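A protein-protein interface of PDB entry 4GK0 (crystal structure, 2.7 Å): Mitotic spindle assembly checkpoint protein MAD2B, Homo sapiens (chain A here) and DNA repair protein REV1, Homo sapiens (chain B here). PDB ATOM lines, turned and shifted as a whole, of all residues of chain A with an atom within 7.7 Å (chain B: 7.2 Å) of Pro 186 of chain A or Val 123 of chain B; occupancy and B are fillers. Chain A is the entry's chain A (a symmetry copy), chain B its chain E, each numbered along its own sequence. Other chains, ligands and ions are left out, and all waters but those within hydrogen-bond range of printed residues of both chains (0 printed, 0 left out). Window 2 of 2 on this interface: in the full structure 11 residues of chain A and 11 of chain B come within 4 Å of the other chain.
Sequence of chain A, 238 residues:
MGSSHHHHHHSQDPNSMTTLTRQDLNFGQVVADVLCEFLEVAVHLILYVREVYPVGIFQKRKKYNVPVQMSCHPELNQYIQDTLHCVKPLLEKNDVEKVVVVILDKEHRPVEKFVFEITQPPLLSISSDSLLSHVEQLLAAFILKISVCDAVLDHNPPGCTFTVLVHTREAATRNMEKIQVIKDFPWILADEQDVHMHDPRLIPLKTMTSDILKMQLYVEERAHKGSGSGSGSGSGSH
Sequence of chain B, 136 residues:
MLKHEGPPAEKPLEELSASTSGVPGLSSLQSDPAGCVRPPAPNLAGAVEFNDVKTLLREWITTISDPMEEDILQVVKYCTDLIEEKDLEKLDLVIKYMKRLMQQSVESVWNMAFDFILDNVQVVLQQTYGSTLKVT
The side-chain amide nitrogen (NE2) of Gln 180 of chain A sits close to the backbone NH (N) of Trp 187 of chain A. O of Val 124 of chain B lies within hydrogen-bond range of OG1 of Thr 128 of chain B, at 3.3 Å.
Of the 12 printed residues of chain A, 5 touch a printed residue of chain B. Hydrophobic or aromatic side chains of chain A within 4 Å of the printed part of chain B: Met 176, Pro 186 and Ile 188.
Among the printed residues, pairs that only touch across the chains: Asp 184 of chain A with Gln 127 of chain B, Pro 186 of chain A with Val 123 of chain B, Pro 186 of chain A with Gln 127 of chain B and Ile 188 of chain A with Val 124 of chain B.
The side-chain sulfur of Met 176 of chain A lies close to the side-chain amide oxygen of Asn 120 of chain B (3.4 Å). The side-chain amide oxygen (OE1) of Gln 180 of chain A lies close to the side-chain amide oxygen (OD1) of Asn 120 of chain B.
Of chain B, only Val 123 (3.6 Å) and Gln 127 (3.7 Å) come within 4 Å of Pro 186 of chain A. Val 123 of chain B touches one residue of chain A. Printed residues of chain A within 4 Å of Asn 120 of chain B: Met 176 and Gln 180. Printed residues of chain A within 4 Å of Val 124 of chain B: Ile 188 (3.8 Å). Of the printed residues of chain B, Ile 188 of chain A touches Val 124. Of the printed residues of chain B, Met 176 of chain A touches Asn 120. The nearest printed residue of chain B that does not touch Met 176 of chain A is Val 121 of chain B (7.6 Å).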
ATOM      1  N   CYS A  86       6.770 -24.024  14.075  1.00  0.00           N
ATOM      2  CA  CYS A  86       5.551 -24.603  13.521  1.00  0.00           C
ATOM      3  C   CYS A  86       5.748 -25.428  12.261  1.00  0.00           C
ATOM      4  O   CYS A  86       4.933 -26.296  11.972  1.00  0.00           O
ATOM      5  CB  CYS A  86       4.541 -23.502  13.188  1.00  0.00           C
ATOM      6  SG  CYS A  86       4.012 -22.491  14.564  1.00  0.00           S
ATOM      7  N   MET A 176      -2.323 -28.722   8.561  1.00  0.00           N
ATOM      8  CA  MET A 176      -2.908 -27.766   9.506  1.00  0.00           C
ATOM      9  C   MET A 176      -2.944 -28.204  10.950  1.00  0.00           C
ATOM     10  O   MET A 176      -2.621 -27.437  11.805  1.00  0.00           O
ATOM     11  CB  MET A 176      -4.290 -27.351   9.095  1.00  0.00           C
ATOM     12  CG  MET A 176      -4.295 -26.245   8.070  1.00  0.00           C
ATOM     13  SD  MET A 176      -5.543 -25.002   8.489  1.00  0.00           S
ATOM     14  CE  MET A 176      -5.978 -24.516   6.824  1.00  0.00           C
ATOM     15  N   ILE A 179       0.722 -27.865  12.004  1.00  0.00           N
ATOM     16  CA  ILE A 179       1.236 -26.501  12.024  1.00  0.00           C
ATOM     17  C   ILE A 179       0.675 -25.652  13.156  1.00  0.00           C
ATOM     18  O   ILE A 179       1.261 -24.685  13.583  1.00  0.00           O
ATOM     19  CB  ILE A 179       0.998 -25.791  10.676  1.00  0.00           C
ATOM     20  CG1 ILE A 179       2.111 -24.759  10.443  1.00  0.00           C
ATOM     21  CG2 ILE A 179      -0.397 -25.205  10.616  1.00  0.00           C
ATOM     22  CD1 ILE A 179       2.442 -24.517   8.976  1.00  0.00           C
ATOM     23  N   GLN A 180      -0.473 -26.058  13.653  1.00  0.00           N
ATOM     24  CA  GLN A 180      -1.307 -25.196  14.457  1.00  0.00           C
ATOM     25  C   GLN A 180      -0.968 -25.418  15.923  1.00  0.00           C
ATOM     26  O   GLN A 180      -1.827 -25.601  16.738  1.00  0.00           O
ATOM     27  CB  GLN A 180      -2.755 -25.491  14.087  1.00  0.00           C
ATOM     28  CG  GLN A 180      -3.685 -24.333  14.123  1.00  0.00           C
ATOM     29  CD  GLN A 180      -3.366 -23.245  13.112  1.00  0.00           C
ATOM     30  OE1 GLN A 180      -3.965 -23.166  12.042  1.00  0.00           O
ATOM     31  NE2 GLN A 180      -2.445 -22.374  13.477  1.00  0.00           N
ATOM     32  N   VAL A 181       0.311 -25.342  16.251  1.00  0.00           N
ATOM     33  CA  VAL A 181       0.814 -25.717  17.575  1.00  0.00           C
ATOM     34  C   VAL A 181       1.054 -24.648  18.595  1.00  0.00           C
ATOM     35  O   VAL A 181       1.312 -24.971  19.735  1.00  0.00           O
ATOM     36  CB  VAL A 181       2.138 -26.503  17.503  1.00  0.00           C
ATOM     37  CG1 VAL A 181       1.838 -28.007  17.469  1.00  0.00           C
ATOM     38  CG2 VAL A 181       2.995 -26.069  16.326  1.00  0.00           C
ATOM     39  N   ILE A 182       1.007 -23.386  18.215  1.00  0.00           N
ATOM     40  CA  ILE A 182       1.142 -22.272  19.146  1.00  0.00           C
ATOM     41  C   ILE A 182      -0.139 -21.466  19.036  1.00  0.00           C
ATOM     42  O   ILE A 182      -0.397 -20.883  18.007  1.00  0.00           O
ATOM     43  CB  ILE A 182       2.371 -21.410  18.792  1.00  0.00           C
ATOM     44  CG1 ILE A 182       3.651 -22.248  18.784  1.00  0.00           C
ATOM     45  CG2 ILE A 182       2.566 -20.282  19.772  1.00  0.00           C
ATOM     46  CD1 ILE A 182       4.887 -21.503  18.287  1.00  0.00           C
ATOM     47  N   LYS A 183      -0.965 -21.478  20.074  1.00  0.00           N
ATOM     48  CA  LYS A 183      -2.229 -20.719  20.098  1.00  0.00           C
ATOM     49  C   LYS A 183      -1.996 -19.282  19.682  1.00  0.00           C
ATOM     50  O   LYS A 183      -2.653 -18.777  18.792  1.00  0.00           O
ATOM     51  CB  LYS A 183      -2.864 -20.689  21.495  1.00  0.00           C
ATOM     52  CG  LYS A 183      -2.134 -21.456  22.593  1.00  0.00           C
ATOM     53  CD  LYS A 183      -3.048 -21.819  23.768  1.00  0.00           C
ATOM     54  CE  LYS A 183      -2.411 -22.898  24.663  1.00  0.00           C
ATOM     55  NZ  LYS A 183      -3.383 -23.909  25.181  1.00  0.00           N
ATOM     56  N   ASP A 184      -1.048 -18.633  20.351  1.00  0.00           N
ATOM     57  CA  ASP A 184      -0.633 -17.260  20.028  1.00  0.00           C
ATOM     58  C   ASP A 184      -0.201 -17.054  18.581  1.00  0.00           C
ATOM     59  O   ASP A 184      -0.206 -15.935  18.099  1.00  0.00           O
ATOM     60  CB  ASP A 184       0.565 -16.877  20.914  1.00  0.00           C
ATOM     61  CG  ASP A 184       0.152 -16.372  22.292  1.00  0.00           C
ATOM     62  OD1 ASP A 184      -1.057 -16.433  22.637  1.00  0.00           O
ATOM     63  OD2 ASP A 184       1.060 -15.914  23.026  1.00  0.00           O
ATOM     64  N   PHE A 185       0.193 -18.124  17.895  1.00  0.00           N
ATOM     65  CA  PHE A 185       0.744 -18.005  16.552  1.00  0.00           C
ATOM     66  C   PHE A 185       0.076 -18.919  15.512  1.00  0.00           C
ATOM     67  O   PHE A 185       0.687 -19.847  15.015  1.00  0.00           O
ATOM     68  CB  PHE A 185       2.265 -18.248  16.605  1.00  0.00           C
ATOM     69  CG  PHE A 185       3.021 -17.620  15.463  1.00  0.00           C
ATOM     70  CD1 PHE A 185       3.384 -16.301  15.511  1.00  0.00           C
ATOM     71  CD2 PHE A 185       3.361 -18.361  14.347  1.00  0.00           C
ATOM     72  CE1 PHE A 185       4.047 -15.710  14.468  1.00  0.00           C
ATOM     73  CE2 PHE A 185       4.037 -17.776  13.294  1.00  0.00           C
ATOM     74  CZ  PHE A 185       4.384 -16.444  13.364  1.00  0.00           C
ATOM     75  N   PRO A 186      -1.161 -18.630  15.129  1.00  0.00           N
ATOM     76  CA  PRO A 186      -1.912 -19.343  14.118  1.00  0.00           C
ATOM     77  C   PRO A 186      -1.573 -19.099  12.660  1.00  0.00           C
ATOM     78  O   PRO A 186      -0.985 -18.085  12.311  1.00  0.00           O
ATOM     79  CB  PRO A 186      -3.341 -18.846  14.313  1.00  0.00           C
ATOM     80  CG  PRO A 186      -3.312 -17.893  15.449  1.00  0.00           C
ATOM     81  CD  PRO A 186      -1.903 -17.488  15.655  1.00  0.00           C
ATOM     82  N   TRP A 187      -2.075 -19.991  11.814  1.00  0.00           N
ATOM     83  CA  TRP A 187      -1.747 -20.069  10.406  1.00  0.00           C
ATOM     84  C   TRP A 187      -3.047 -20.087   9.629  1.00  0.00           C
ATOM     85  O   TRP A 187      -4.054 -20.575  10.097  1.00  0.00           O
ATOM     86  CB  TRP A 187      -0.938 -21.333  10.073  1.00  0.00           C
ATOM     87  CG  TRP A 187       0.461 -21.299  10.548  1.00  0.00           C
ATOM     88  CD1 TRP A 187       0.874 -21.352  11.833  1.00  0.00           C
ATOM     89  CD2 TRP A 187       1.653 -21.192   9.763  1.00  0.00           C
ATOM     90  NE1 TRP A 187       2.241 -21.309  11.906  1.00  0.00           N
ATOM     91  CE2 TRP A 187       2.736 -21.211  10.637  1.00  0.00           C
ATOM     92  CE3 TRP A 187       1.910 -21.097   8.401  1.00  0.00           C
ATOM     93  CZ2 TRP A 187       4.045 -21.106  10.195  1.00  0.00           C
ATOM     94  CZ3 TRP A 187       3.213 -21.000   7.970  1.00  0.00           C
ATOM     95  CH2 TRP A 187       4.257 -20.999   8.860  1.00  0.00           C
ATOM     96  N   ILE A 188      -3.015 -19.563   8.417  1.00  0.00           N
ATOM     97  CA  ILE A 188      -4.164 -19.635   7.561  1.00  0.00           C
ATOM     98  C   ILE A 188      -3.703 -20.133   6.234  1.00  0.00           C
ATOM     99  O   ILE A 188      -2.514 -20.173   5.991  1.00  0.00           O
ATOM    100  CB  ILE A 188      -4.827 -18.281   7.382  1.00  0.00           C
ATOM    101  CG1 ILE A 188      -3.827 -17.277   6.837  1.00  0.00           C
ATOM    102  CG2 ILE A 188      -5.444 -17.872   8.690  1.00  0.00           C
ATOM    103  CD1 ILE A 188      -4.420 -15.925   6.556  1.00  0.00           C
ATOM    104  N   ILE B  83     -13.618 -13.821   8.311  1.00  0.00           N
ATOM    105  CA  ILE B  83     -13.106 -13.051   9.453  1.00  0.00           C
ATOM    106  C   ILE B  83     -12.325 -11.831   8.974  1.00  0.00           C
ATOM    107  O   ILE B  83     -12.573 -10.731   9.436  1.00  0.00           O
ATOM    108  CB  ILE B  83     -12.238 -13.863  10.373  1.00  0.00           C
ATOM    109  CG1 ILE B  83     -13.093 -14.894  11.112  1.00  0.00           C
ATOM    110  CG2 ILE B  83     -11.514 -12.929  11.339  1.00  0.00           C
ATOM    111  CD1 ILE B  83     -12.266 -16.004  11.770  1.00  0.00           C
ATOM    112  N   LEU B 118     -13.678 -25.891  13.044  1.00  0.00           N
ATOM    113  CA  LEU B 118     -14.028 -24.955  14.116  1.00  0.00           C
ATOM    114  C   LEU B 118     -12.772 -24.616  14.847  1.00  0.00           C
ATOM    115  O   LEU B 118     -12.558 -23.480  15.181  1.00  0.00           O
ATOM    116  CB  LEU B 118     -15.073 -25.526  15.094  1.00  0.00           C
ATOM    117  CG  LEU B 118     -15.524 -24.658  16.287  1.00  0.00           C
ATOM    118  CD1 LEU B 118     -16.356 -23.450  15.906  1.00  0.00           C
ATOM    119  CD2 LEU B 118     -16.284 -25.446  17.331  1.00  0.00           C
ATOM    120  N   ASP B 119     -11.955 -25.615  15.128  1.00  0.00           N
ATOM    121  CA  ASP B 119     -10.662 -25.386  15.736  1.00  0.00           C
ATOM    122  C   ASP B 119      -9.950 -24.300  14.977  1.00  0.00           C
ATOM    123  O   ASP B 119      -9.511 -23.325  15.562  1.00  0.00           O
ATOM    124  CB  ASP B 119      -9.807 -26.634  15.643  1.00  0.00           C
ATOM    125  CG  ASP B 119     -10.111 -27.649  16.699  1.00  0.00           C
ATOM    126  OD1 ASP B 119     -10.984 -27.449  17.558  1.00  0.00           O
ATOM    127  OD2 ASP B 119      -9.441 -28.704  16.665  1.00  0.00           O
ATOM    128  N   ASN B 120      -9.828 -24.478  13.669  1.00  0.00           N
ATOM    129  CA  ASN B 120      -9.034 -23.562  12.861  1.00  0.00           C
ATOM    130  C   ASN B 120      -9.668 -22.176  12.721  1.00  0.00           C
ATOM    131  O   ASN B 120      -8.999 -21.229  12.392  1.00  0.00           O
ATOM    132  CB  ASN B 120      -8.720 -24.167  11.489  1.00  0.00           C
ATOM    133  CG  ASN B 120      -7.663 -25.228  11.572  1.00  0.00           C
ATOM    134  OD1 ASN B 120      -6.521 -24.913  11.784  1.00  0.00           O
ATOM    135  ND2 ASN B 120      -8.037 -26.492  11.437  1.00  0.00           N
ATOM    136  N   VAL B 121     -10.960 -22.065  12.971  1.00  0.00           N
ATOM    137  CA  VAL B 121     -11.621 -20.794  12.954  1.00  0.00           C
ATOM    138  C   VAL B 121     -11.413 -20.143  14.315  1.00  0.00           C
ATOM    139  O   VAL B 121     -11.172 -18.955  14.417  1.00  0.00           O
ATOM    140  CB  VAL B 121     -13.115 -20.992  12.626  1.00  0.00           C
ATOM    141  CG1 VAL B 121     -13.971 -19.777  12.991  1.00  0.00           C
ATOM    142  CG2 VAL B 121     -13.256 -21.308  11.155  1.00  0.00           C
ATOM    143  N   GLN B 122     -11.489 -20.919  15.371  1.00  0.00           N
ATOM    144  CA  GLN B 122     -11.271 -20.370  16.692  1.00  0.00           C
ATOM    145  C   GLN B 122      -9.888 -19.741  16.943  1.00  0.00           C
ATOM    146  O   GLN B 122      -9.799 -18.671  17.553  1.00  0.00           O
ATOM    147  CB  GLN B 122     -11.612 -21.395  17.783  1.00  0.00           C
ATOM    148  CG  GLN B 122     -13.051 -21.927  17.731  1.00  0.00           C
ATOM    149  CD  GLN B 122     -14.110 -20.949  18.231  1.00  0.00           C
ATOM    150  OE1 GLN B 122     -14.186 -19.812  17.787  1.00  0.00           O
ATOM    151  NE2 GLN B 122     -14.951 -21.400  19.121  1.00  0.00           N
ATOM    152  N   VAL B 123      -8.803 -20.345  16.478  1.00  0.00           N
ATOM    153  CA  VAL B 123      -7.504 -19.759  16.797  1.00  0.00           C
ATOM    154  C   VAL B 123      -7.384 -18.462  16.054  1.00  0.00           C
ATOM    155  O   VAL B 123      -6.764 -17.532  16.541  1.00  0.00           O
ATOM    156  CB  VAL B 123      -6.286 -20.663  16.491  1.00  0.00           C
ATOM    157  CG1 VAL B 123      -6.315 -21.893  17.338  1.00  0.00           C
ATOM    158  CG2 VAL B 123      -6.263 -21.107  15.051  1.00  0.00           C
ATOM    159  N   VAL B 124      -7.992 -18.379  14.881  1.00  0.00           N
ATOM    160  CA  VAL B 124      -7.963 -17.142  14.128  1.00  0.00           C
ATOM    161  C   VAL B 124      -8.833 -16.090  14.809  1.00  0.00           C
ATOM    162  O   VAL B 124      -8.377 -14.962  14.984  1.00  0.00           O
ATOM    163  CB  VAL B 124      -8.346 -17.308  12.645  1.00  0.00           C
ATOM    164  CG1 VAL B 124      -8.282 -15.946  11.962  1.00  0.00           C
ATOM    165  CG2 VAL B 124      -7.407 -18.280  11.946  1.00  0.00           C
ATOM    166  N   LEU B 125     -10.048 -16.416  15.233  1.00  0.00           N
ATOM    167  CA  LEU B 125     -10.822 -15.386  15.933  1.00  0.00           C
ATOM    168  C   LEU B 125     -10.127 -14.900  17.181  1.00  0.00           C
ATOM    169  O   LEU B 125     -10.112 -13.729  17.467  1.00  0.00           O
ATOM    170  CB  LEU B 125     -12.203 -15.863  16.329  1.00  0.00           C
ATOM    171  CG  LEU B 125     -13.150 -15.835  15.161  1.00  0.00           C
ATOM    172  CD1 LEU B 125     -14.317 -16.762  15.511  1.00  0.00           C
ATOM    173  CD2 LEU B 125     -13.593 -14.420  14.912  1.00  0.00           C
ATOM    174  N   GLN B 126      -9.544 -15.823  17.926  1.00  0.00           N
ATOM    175  CA  GLN B 126      -8.958 -15.512  19.236  1.00  0.00           C
ATOM    176  C   GLN B 126      -7.857 -14.507  19.075  1.00  0.00           C
ATOM    177  O   GLN B 126      -7.569 -13.778  19.991  1.00  0.00           O
ATOM    178  CB  GLN B 126      -8.484 -16.783  19.932  1.00  0.00           C
ATOM    179  CG  GLN B 126      -7.633 -16.615  21.179  1.00  0.00           C
ATOM    180  CD  GLN B 126      -8.406 -16.009  22.343  1.00  0.00           C
ATOM    181  OE1 GLN B 126      -9.201 -16.692  22.997  1.00  0.00           O
ATOM    182  NE2 GLN B 126      -8.152 -14.711  22.626  1.00  0.00           N
ATOM    183  N   GLN B 127      -7.272 -14.434  17.882  1.00  0.00           N
ATOM    184  CA  GLN B 127      -6.228 -13.435  17.577  1.00  0.00           C
ATOM    185  C   GLN B 127      -6.725 -12.251  16.797  1.00  0.00           C
ATOM    186  O   GLN B 127      -6.101 -11.236  16.821  1.00  0.00           O
ATOM    187  CB  GLN B 127      -5.123 -14.075  16.751  1.00  0.00           C
ATOM    188  CG  GLN B 127      -4.339 -15.084  17.550  1.00  0.00           C
ATOM    189  CD  GLN B 127      -3.712 -14.442  18.752  1.00  0.00           C
ATOM    190  OE1 GLN B 127      -3.974 -14.855  19.883  1.00  0.00           O
ATOM    191  NE2 GLN B 127      -2.878 -13.427  18.515  1.00  0.00           N
ATOM    192  N   THR B 128      -7.795 -12.375  16.029  1.00  0.00           N
ATOM    193  CA  THR B 128      -8.270 -11.208  15.342  1.00  0.00           C
ATOM    194  C   THR B 128      -9.152 -10.373  16.247  1.00  0.00           C
ATOM    195  O   THR B 128      -9.213  -9.160  16.101  1.00  0.00           O
ATOM    196  CB  THR B 128      -8.972 -11.554  14.035  1.00  0.00           C
ATOM    197  OG1 THR B 128      -8.035 -12.181  13.174  1.00  0.00           O
ATOM    198  CG2 THR B 128      -9.432 -10.287  13.306  1.00  0.00           C
ATOM    199  N   SER B 131     -11.213 -13.351  21.138  1.00  0.00           N
ATOM    200  CA  SER B 131     -12.440 -14.061  21.515  1.00  0.00           C
ATOM    201  C   SER B 131     -12.616 -15.283  20.663  1.00  0.00           C
ATOM    202  O   SER B 131     -12.176 -15.294  19.542  1.00  0.00           O
ATOM    203  CB  SER B 131     -13.645 -13.187  21.205  1.00  0.00           C
ATOM    204  OG  SER B 131     -14.086 -12.528  22.356  1.00  0.00           O
ATOM    205  N   THR B 132     -13.328 -16.279  21.177  1.00  0.00           N
ATOM    206  CA  THR B 132     -13.691 -17.421  20.378  1.00  0.00           C
ATOM    207  C   THR B 132     -15.181 -17.403  20.199  1.00  0.00           C
ATOM    208  O   THR B 132     -15.861 -16.870  21.010  1.00  0.00           O
ATOM    209  CB  THR B 132     -13.232 -18.738  21.016  1.00  0.00           C
ATOM    210  OG1 THR B 132     -13.720 -18.818  22.353  1.00  0.00           O
ATOM    211  CG2 THR B 132     -11.707 -18.803  21.030  1.00  0.00           C
